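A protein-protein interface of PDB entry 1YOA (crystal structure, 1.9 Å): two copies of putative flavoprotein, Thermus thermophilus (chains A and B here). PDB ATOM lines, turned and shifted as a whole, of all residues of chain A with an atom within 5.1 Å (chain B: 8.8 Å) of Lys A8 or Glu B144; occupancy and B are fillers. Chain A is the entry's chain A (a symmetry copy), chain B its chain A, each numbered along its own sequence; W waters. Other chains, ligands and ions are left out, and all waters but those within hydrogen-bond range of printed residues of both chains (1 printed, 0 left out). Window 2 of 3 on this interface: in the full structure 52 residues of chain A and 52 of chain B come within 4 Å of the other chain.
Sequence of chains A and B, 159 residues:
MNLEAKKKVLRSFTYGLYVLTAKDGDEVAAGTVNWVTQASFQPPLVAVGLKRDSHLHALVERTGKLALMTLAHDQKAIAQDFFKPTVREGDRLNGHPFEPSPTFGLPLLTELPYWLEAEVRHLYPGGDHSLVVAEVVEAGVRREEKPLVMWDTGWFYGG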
ATOM      1  N   GLU A   4       7.017  -7.352   1.269  1.00  0.00           N
ATOM      2  CA  GLU A   4       5.844  -6.978   2.046  1.00  0.00           C
ATOM      3  C   GLU A   4       5.153  -5.775   1.395  1.00  0.00           C
ATOM      4  O   GLU A   4       3.929  -5.738   1.289  1.00  0.00           O
ATOM      5  CB  GLU A   4       6.191  -6.702   3.512  1.00  0.00           C
ATOM      6  CG  GLU A   4       6.050  -7.951   4.373  1.00  0.00           C
ATOM      7  CD  GLU A   4       4.589  -8.312   4.634  1.00  0.00           C
ATOM      8  OE1 GLU A   4       3.952  -7.641   5.496  1.00  0.00           O
ATOM      9  OE2 GLU A   4       4.064  -9.256   3.973  1.00  0.00           O
ATOM     10  N   ALA A   5       5.951  -4.818   0.938  1.00  0.00           N
ATOM     11  CA  ALA A   5       5.426  -3.619   0.310  1.00  0.00           C
ATOM     12  C   ALA A   5       4.763  -3.927  -1.042  1.00  0.00           C
ATOM     13  O   ALA A   5       3.721  -3.373  -1.341  1.00  0.00           O
ATOM     14  CB  ALA A   5       6.548  -2.544   0.138  1.00  0.00           C
ATOM     15  N   LYS A   6       5.384  -4.763  -1.859  1.00  0.00           N
ATOM     16  CA  LYS A   6       4.805  -5.192  -3.142  1.00  0.00           C
ATOM     17  C   LYS A   6       3.409  -5.808  -2.954  1.00  0.00           C
ATOM     18  O   LYS A   6       2.464  -5.497  -3.708  1.00  0.00           O
ATOM     19  CB  LYS A   6       5.721  -6.180  -3.833  1.00  0.00           C
ATOM     20  CG  LYS A   6       5.214  -6.747  -5.140  1.00  0.00           C
ATOM     21  CD  LYS A   6       4.527  -8.100  -4.956  1.00  0.00           C
ATOM     22  CE  LYS A   6       5.524  -9.214  -4.730  1.00  0.00           C
ATOM     23  NZ  LYS A   6       4.821 -10.518  -4.719  1.00  0.00           N
ATOM     24  N   LYS A   7       3.281  -6.669  -1.939  1.00  0.00           N
ATOM     25  CA  LYS A   7       1.989  -7.292  -1.647  1.00  0.00           C
ATOM     26  C   LYS A   7       0.946  -6.274  -1.283  1.00  0.00           C
ATOM     27  O   LYS A   7      -0.183  -6.348  -1.787  1.00  0.00           O
ATOM     28  CB  LYS A   7       2.086  -8.330  -0.509  1.00  0.00           C
ATOM     29  CG  LYS A   7       2.997  -9.480  -0.813  1.00  0.00           C
ATOM     30  CD  LYS A   7       3.062 -10.555   0.340  1.00  0.00           C
ATOM     31  CE  LYS A   7       4.526 -10.844   0.787  1.00  0.00           C
ATOM     32  NZ  LYS A   7       4.648 -11.130   2.265  1.00  0.00           N
ATOM     33  N   LYS A   8       1.305  -5.343  -0.388  1.00  0.00           N
ATOM     34  CA  LYS A   8       0.401  -4.294   0.051  1.00  0.00           C
ATOM     35  C   LYS A   8       0.023  -3.338  -1.089  1.00  0.00           C
ATOM     36  O   LYS A   8      -1.127  -2.941  -1.193  1.00  0.00           O
ATOM     37  CB  LYS A   8       0.965  -3.525   1.223  1.00  0.00           C
ATOM     38  CG  LYS A   8       0.794  -4.246   2.575  1.00  0.00           C
ATOM     39  CD  LYS A   8       1.648  -3.590   3.648  1.00  0.00           C
ATOM     40  CE  LYS A   8       1.745  -4.453   4.913  1.00  0.00           C
ATOM     41  NZ  LYS A   8       3.090  -4.316   5.529  1.00  0.00           N
ATOM     42  N   VAL A   9       0.992  -3.013  -1.946  1.00  0.00           N
ATOM     43  CA  VAL A   9       0.741  -2.146  -3.095  1.00  0.00           C
ATOM     44  C   VAL A   9      -0.236  -2.796  -4.073  1.00  0.00           C
ATOM     45  O   VAL A   9      -1.216  -2.174  -4.457  1.00  0.00           O
ATOM     46  CB  VAL A   9       2.069  -1.737  -3.755  1.00  0.00           C
ATOM     47  CG1 VAL A   9       1.841  -1.026  -5.061  1.00  0.00           C
ATOM     48  CG2 VAL A   9       2.818  -0.817  -2.787  1.00  0.00           C
ATOM     49  N   LEU A  10      -0.016  -4.062  -4.420  1.00  0.00           N
ATOM     50  CA  LEU A  10      -0.892  -4.738  -5.384  1.00  0.00           C
ATOM     51  C   LEU A  10      -2.295  -4.935  -4.788  1.00  0.00           C
ATOM     52  O   LEU A  10      -3.283  -4.872  -5.508  1.00  0.00           O
ATOM     53  CB  LEU A  10      -0.273  -6.038  -5.904  1.00  0.00           C
ATOM     54  CG  LEU A  10       0.990  -5.929  -6.777  1.00  0.00           C
ATOM     55  CD1 LEU A  10       1.623  -7.279  -7.104  1.00  0.00           C
ATOM     56  CD2 LEU A  10       0.713  -5.171  -8.089  1.00  0.00           C
ATOM     57  N   ARG A  11      -2.377  -5.142  -3.472  1.00  0.00           N
ATOM     58  CA  ARG A  11      -3.659  -5.244  -2.782  1.00  0.00           C
ATOM     59  C   ARG A  11      -4.375  -3.907  -2.597  1.00  0.00           C
ATOM     60  O   ARG A  11      -5.503  -3.886  -2.160  1.00  0.00           O
ATOM     61  CB  ARG A  11      -3.487  -5.960  -1.435  1.00  0.00           C
ATOM     62  CG  ARG A  11      -3.137  -7.386  -1.648  1.00  0.00           C
ATOM     63  CD  ARG A  11      -3.180  -8.242  -0.413  1.00  0.00           C
ATOM     64  NE  ARG A  11      -2.964  -9.626  -0.811  1.00  0.00           N
ATOM     65  CZ  ARG A  11      -3.122 -10.683  -0.015  1.00  0.00           C
ATOM     66  NH1 ARG A  11      -2.885 -11.905  -0.497  1.00  0.00           N
ATOM     67  NH2 ARG A  11      -3.485 -10.532   1.253  1.00  0.00           N
ATOM     68  N   SER A  12      -3.744  -2.786  -2.965  1.00  0.00           N
ATOM     69  CA  SER A  12      -4.443  -1.488  -2.951  1.00  0.00           C
ATOM     70  C   SER A  12      -5.249  -1.235  -4.243  1.00  0.00           C
ATOM     71  O   SER A  12      -5.944  -0.226  -4.338  1.00  0.00           O
ATOM     72  CB  SER A  12      -3.449  -0.332  -2.740  1.00  0.00           C
ATOM     73  OG  SER A  12      -2.700  -0.054  -3.916  1.00  0.00           O
ATOM     74  N   GLN B  38      -3.759  -6.263 -11.943  1.00  0.00           N
ATOM     75  CA  GLN B  38      -2.702  -7.256 -11.800  1.00  0.00           C
ATOM     76  C   GLN B  38      -2.938  -8.343 -12.896  1.00  0.00           C
ATOM     77  O   GLN B  38      -4.079  -8.551 -13.354  1.00  0.00           O
ATOM     78  CB  GLN B  38      -2.684  -7.788 -10.356  1.00  0.00           C
ATOM     79  CG  GLN B  38      -1.578  -8.774 -10.085  1.00  0.00           C
ATOM     80  CD  GLN B  38      -1.309  -9.086  -8.639  1.00  0.00           C
ATOM     81  OE1 GLN B  38      -0.438  -9.969  -8.363  1.00  0.00           O
ATOM     82  NE2 GLN B  38      -2.039  -8.495  -7.733  1.00  0.00           N
ATOM     83  N   THR B  70      -0.955   4.499  -6.291  1.00  0.00           N
ATOM     84  CA  THR B  70      -2.371   4.475  -5.953  1.00  0.00           C
ATOM     85  C   THR B  70      -2.813   5.717  -5.223  1.00  0.00           C
ATOM     86  O   THR B  70      -2.298   6.041  -4.173  1.00  0.00           O
ATOM     87  CB  THR B  70      -2.676   3.263  -5.059  1.00  0.00           C
ATOM     88  OG1 THR B  70      -2.127   2.084  -5.662  1.00  0.00           O
ATOM     89  CG2 THR B  70      -4.209   3.030  -4.930  1.00  0.00           C
ATOM     90  N   ALA B  72      -5.066   7.767  -2.706  1.00  0.00           N
ATOM     91  CA  ALA B  72      -5.914   7.612  -1.523  1.00  0.00           C
ATOM     92  C   ALA B  72      -7.333   8.109  -1.711  1.00  0.00           C
ATOM     93  O   ALA B  72      -7.619   8.951  -2.557  1.00  0.00           O
ATOM     94  CB  ALA B  72      -5.271   8.337  -0.293  1.00  0.00           C
ATOM     95  N   HIS B  73      -8.222   7.637  -0.845  1.00  0.00           N
ATOM     96  CA  HIS B  73      -9.641   7.985  -0.882  1.00  0.00           C
ATOM     97  C   HIS B  73      -9.906   9.509  -0.845  1.00  0.00           C
ATOM     98  O   HIS B  73     -10.898   9.961  -1.382  1.00  0.00           O
ATOM     99  CB  HIS B  73     -10.376   7.295   0.293  1.00  0.00           C
ATOM    100  CG  HIS B  73      -9.941   7.794   1.639  1.00  0.00           C
ATOM    101  ND1 HIS B  73     -10.513   8.890   2.246  1.00  0.00           N
ATOM    102  CD2 HIS B  73      -8.972   7.364   2.482  1.00  0.00           C
ATOM    103  CE1 HIS B  73      -9.920   9.115   3.409  1.00  0.00           C
ATOM    104  NE2 HIS B  73      -8.966   8.216   3.568  1.00  0.00           N
ATOM    105  N   PRO B 113      -0.054   7.069  -1.109  1.00  0.00           N
ATOM    106  CA  PRO B 113       0.362   6.071  -0.105  1.00  0.00           C
ATOM    107  C   PRO B 113       1.075   4.790  -0.609  1.00  0.00           C
ATOM    108  O   PRO B 113       1.795   4.131   0.168  1.00  0.00           O
ATOM    109  CB  PRO B 113      -0.964   5.752   0.637  1.00  0.00           C
ATOM    110  CG  PRO B 113      -2.054   6.045  -0.340  1.00  0.00           C
ATOM    111  CD  PRO B 113      -1.510   7.207  -1.195  1.00  0.00           C
ATOM    112  N   TYR B 114       0.884   4.427  -1.881  1.00  0.00           N
ATOM    113  CA  TYR B 114       1.378   3.184  -2.436  1.00  0.00           C
ATOM    114  C   TYR B 114       2.036   3.476  -3.763  1.00  0.00           C
ATOM    115  O   TYR B 114       1.493   4.282  -4.541  1.00  0.00           O
ATOM    116  CB  TYR B 114       0.220   2.192  -2.704  1.00  0.00           C
ATOM    117  CG  TYR B 114      -0.589   1.793  -1.504  1.00  0.00           C
ATOM    118  CD1 TYR B 114      -0.139   0.792  -0.635  1.00  0.00           C
ATOM    119  CD2 TYR B 114      -1.821   2.370  -1.251  1.00  0.00           C
ATOM    120  CE1 TYR B 114      -0.890   0.411   0.481  1.00  0.00           C
ATOM    121  CE2 TYR B 114      -2.580   1.982  -0.152  1.00  0.00           C
ATOM    122  CZ  TYR B 114      -2.091   0.998   0.713  1.00  0.00           C
ATOM    123  OH  TYR B 114      -2.848   0.614   1.792  1.00  0.00           O
ATOM    124  N   TRP B 115       3.195   2.882  -3.992  1.00  0.00           N
ATOM    125  CA  TRP B 115       3.892   3.002  -5.265  1.00  0.00           C
ATOM    126  C   TRP B 115       4.620   1.759  -5.659  1.00  0.00           C
ATOM    127  O   TRP B 115       5.012   0.950  -4.799  1.00  0.00           O
ATOM    128  CB  TRP B 115       4.858   4.218  -5.274  1.00  0.00           C
ATOM    129  CG  TRP B 115       6.058   4.055  -4.365  1.00  0.00           C
ATOM    130  CD1 TRP B 115       6.185   4.545  -3.109  1.00  0.00           C
ATOM    131  CD2 TRP B 115       7.266   3.355  -4.644  1.00  0.00           C
ATOM    132  NE1 TRP B 115       7.395   4.180  -2.575  1.00  0.00           N
ATOM    133  CE2 TRP B 115       8.083   3.451  -3.493  1.00  0.00           C
ATOM    134  CE3 TRP B 115       7.758   2.657  -5.748  1.00  0.00           C
ATOM    135  CZ2 TRP B 115       9.347   2.883  -3.423  1.00  0.00           C
ATOM    136  CZ3 TRP B 115       8.997   2.083  -5.671  1.00  0.00           C
ATOM    137  CH2 TRP B 115       9.788   2.207  -4.503  1.00  0.00           C
ATOM    138  N   LEU B 116       4.799   1.591  -6.975  1.00  0.00           N
ATOM    139  CA  LEU B 116       5.586   0.540  -7.558  1.00  0.00           C
ATOM    140  C   LEU B 116       6.349   1.063  -8.756  1.00  0.00           C
ATOM    141  O   LEU B 116       5.898   1.982  -9.424  1.00  0.00           O
ATOM    142  CB  LEU B 116       4.731  -0.685  -7.979  1.00  0.00           C
ATOM    143  CG  LEU B 116       3.683  -0.477  -9.089  1.00  0.00           C
ATOM    144  CD1 LEU B 116       4.251  -0.648 -10.529  1.00  0.00           C
ATOM    145  CD2 LEU B 116       2.531  -1.453  -8.845  1.00  0.00           C
ATOM    146  N   ALA B 139       8.768  -1.701  -4.787  1.00  0.00           N
ATOM    147  CA  ALA B 139       7.545  -1.067  -4.317  1.00  0.00           C
ATOM    148  C   ALA B 139       7.736  -0.503  -2.926  1.00  0.00           C
ATOM    149  O   ALA B 139       8.689  -0.844  -2.231  1.00  0.00           O
ATOM    150  CB  ALA B 139       6.398  -2.088  -4.313  1.00  0.00           C
ATOM    151  N   GLY B 140       6.841   0.371  -2.542  1.00  0.00           N
ATOM    152  CA  GLY B 140       6.848   0.972  -1.234  1.00  0.00           C
ATOM    153  C   GLY B 140       5.479   1.369  -0.738  1.00  0.00           C
ATOM    154  O   GLY B 140       4.585   1.712  -1.516  1.00  0.00           O
ATOM    155  N   VAL B 141       5.328   1.369   0.585  1.00  0.00           N
ATOM    156  CA  VAL B 141       4.111   1.801   1.260  1.00  0.00           C
ATOM    157  C   VAL B 141       4.471   2.931   2.227  1.00  0.00           C
ATOM    158  O   VAL B 141       5.387   2.778   3.034  1.00  0.00           O
ATOM    159  CB  VAL B 141       3.502   0.617   2.080  1.00  0.00           C
ATOM    160  CG1 VAL B 141       2.286   1.058   2.907  1.00  0.00           C
ATOM    161  CG2 VAL B 141       3.158  -0.528   1.182  1.00  0.00           C
ATOM    162  N   ARG B 142       3.781   4.068   2.152  1.00  0.00           N
ATOM    163  CA  ARG B 142       4.041   5.179   3.070  1.00  0.00           C
ATOM    164  C   ARG B 142       3.132   5.082   4.294  1.00  0.00           C
ATOM    165  O   ARG B 142       3.511   5.458   5.405  1.00  0.00           O
ATOM    166  CB  ARG B 142       3.803   6.517   2.375  1.00  0.00           C
ATOM    167  CG  ARG B 142       4.465   6.598   1.000  1.00  0.00           C
ATOM    168  CD  ARG B 142       4.465   7.995   0.412  1.00  0.00           C
ATOM    169  NE  ARG B 142       5.013   8.005  -0.928  1.00  0.00           N
ATOM    170  CZ  ARG B 142       6.299   8.116  -1.221  1.00  0.00           C
ATOM    171  NH1 ARG B 142       7.217   8.274  -0.265  1.00  0.00           N
ATOM    172  NH2 ARG B 142       6.678   8.090  -2.485  1.00  0.00           N
ATOM    173  N   ARG B 143       1.919   4.601   4.046  1.00  0.00           N
ATOM    174  CA  ARG B 143       0.901   4.334   5.066  1.00  0.00           C
ATOM    175  C   ARG B 143      -0.189   3.458   4.431  1.00  0.00           C
ATOM    176  O   ARG B 143      -0.350   3.459   3.207  1.00  0.00           O
ATOM    177  CB  ARG B 143       0.283   5.625   5.579  1.00  0.00           C
ATOM    178  CG  ARG B 143      -0.436   6.454   4.506  1.00  0.00           C
ATOM    179  CD  ARG B 143      -0.925   7.825   4.953  1.00  0.00           C
ATOM    180  NE  ARG B 143      -1.433   8.615   3.814  1.00  0.00           N
ATOM    181  CZ  ARG B 143      -0.672   9.174   2.869  1.00  0.00           C
ATOM    182  NH1 ARG B 143       0.654   9.049   2.897  1.00  0.00           N
ATOM    183  NH2 ARG B 143      -1.245   9.851   1.872  1.00  0.00           N
ATOM    184  N   GLU B 144      -0.926   2.703   5.235  1.00  0.00           N
ATOM    185  CA  GLU B 144      -2.049   1.937   4.704  1.00  0.00           C
ATOM    186  C   GLU B 144      -3.248   2.843   4.736  1.00  0.00           C
ATOM    187  O   GLU B 144      -3.550   3.457   5.764  1.00  0.00           O
ATOM    188  CB  GLU B 144      -2.262   0.629   5.481  1.00  0.00           C
ATOM    189  CG  GLU B 144      -0.962  -0.142   5.551  1.00  0.00           C
ATOM    190  CD  GLU B 144      -1.108  -1.614   5.849  1.00  0.00           C
ATOM    191  OE1 GLU B 144      -2.044  -2.267   5.312  1.00  0.00           O
ATOM    192  OE2 GLU B 144      -0.229  -2.120   6.594  1.00  0.00           O
ATOM    193  N   GLU B 145      -3.885   3.012   3.581  1.00  0.00           N
ATOM    194  CA  GLU B 145      -5.117   3.775   3.500  1.00  0.00           C
ATOM    195  C   GLU B 145      -6.055   3.193   2.463  1.00  0.00           C
ATOM    196  O   GLU B 145      -5.637   2.459   1.590  1.00  0.00           O
ATOM    197  CB  GLU B 145      -4.846   5.266   3.201  1.00  0.00           C
ATOM    198  CG  GLU B 145      -5.705   6.169   4.101  1.00  0.00           C
ATOM    199  CD  GLU B 145      -5.261   7.610   4.079  1.00  0.00           C
ATOM    200  OE1 GLU B 145      -5.691   8.333   3.141  1.00  0.00           O
ATOM    201  OE2 GLU B 145      -4.489   8.021   4.994  1.00  0.00           O
ATOM    202  N   LYS B 146      -7.326   3.549   2.573  1.00  0.00           N
ATOM    203  CA  LYS B 146      -8.332   3.169   1.594  1.00  0.00           C
ATOM    204  C   LYS B 146      -7.985   3.897   0.293  1.00  0.00           C
ATOM    205  O   LYS B 146      -7.690   5.082   0.346  1.00  0.00           O
ATOM    206  CB  LYS B 146      -9.713   3.632   2.066  1.00  0.00           C
ATOM    207  CG  LYS B 146     -10.183   2.925   3.335  1.00  0.00           C
ATOM    208  CD  LYS B 146     -11.552   3.411   3.734  1.00  0.00           C
ATOM    209  CE  LYS B 146     -12.205   2.462   4.747  1.00  0.00           C
ATOM    210  NZ  LYS B 146     -13.493   3.018   5.239  1.00  0.00           N
ATOM    211  N   PRO B 147      -8.028   3.223  -0.853  1.00  0.00           N
ATOM    212  CA  PRO B 147      -7.743   3.889  -2.133  1.00  0.00           C
ATOM    213  C   PRO B 147      -8.953   4.623  -2.684  1.00  0.00           C
ATOM    214  O   PRO B 147     -10.066   4.483  -2.168  1.00  0.00           O
ATOM    215  CB  PRO B 147      -7.370   2.719  -3.052  1.00  0.00           C
ATOM    216  CG  PRO B 147      -8.229   1.597  -2.537  1.00  0.00           C
ATOM    217  CD  PRO B 147      -8.345   1.793  -1.044  1.00  0.00           C
HETATM  218  O   HOH W   1      -4.079  -6.675  -7.323  1.00  0.00           O
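The side-chain hydroxyl (OG) of Ser A12 sits at hydrogen-bond distance from the side-chain hydroxyl (OG1) of Thr B70 (2.8 Å).
The backbone NH of Thr B70 is in hydrogen-bond range of the backbone carbonyl oxygen of Tyr B114. O of Trp B115 sits at hydrogen-bond distance from N of Gly B140 (3.0 Å). The side-chain amino group (NZ) of Lys A8 lies within salt-bridge range of the side-chain carboxylate (OE1) of Glu A4 (3.4 Å). OH of Tyr B114 is in hydrogen-bond range of N of Glu B145 (3.2 Å). O of Val A9 sits at hydrogen-bond distance from OG of Ser A12 (2.6 Å).
Among the printed residues, pairs that only touch across the chains: Val A9 with Gly B140, Ser A12 with Pro B147, Val A9 with Trp B115, Lys A8 with Glu B144, Ser A12 with Tyr B114, Leu A10 with Gln B38, Ala A5 with Ala B139, Lys A6 with Ala B139, Lys A8 with Val B141, Lys A8 with Tyr B114, Ala A5 with Gly B140, Ala A5 with Val B141, Val A9 with Leu B116, Val A9 with Tyr B114 and Val A9 with Val B141.
Of the printed residues of chain B, Lys A6 touches Ala B139 (3.7 Å). Printed residues of chain A within 4 Å of Leu B116: Val A9 (3.9 Å). Printed residues of chain B within 4 Å of Leu A10: Gln B38 (3.5 Å). Arg B143 touches none of the printed residues of chain A. The nearest printed residue of chain B that does not touch Lys A8 is Thr B70 (6.8 Å). The nearest printed residue of chain A that does not touch Glu B144 is Glu A4 (7.0 Å).
Of the 9 printed residues of chain A, 6 touch a printed residue of chain B. Printed residues of chain A that touch a printed residue of chain B: Ala A5, Lys A6, Lys A8, Val A9, Leu A10 and Ser A12. Along chain A the printed residues that touch a printed residue of chain B span positions 5 to 12. Hydrophobic or aromatic side chains of chain B that line the printed part of chain A: Tyr B114, Leu B116, Ala B139, Val B141 and Pro B147. Among the printed residues, 16 pairs touch across the chains.
No position is printed for both chains.
Water W1 lies within hydrogen-bond range of the backbone carbonyl oxygen (O) of Leu A10 (2.7 Å) and the side-chain amide nitrogen (NE2) of Gln B38 (2.8 Å).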
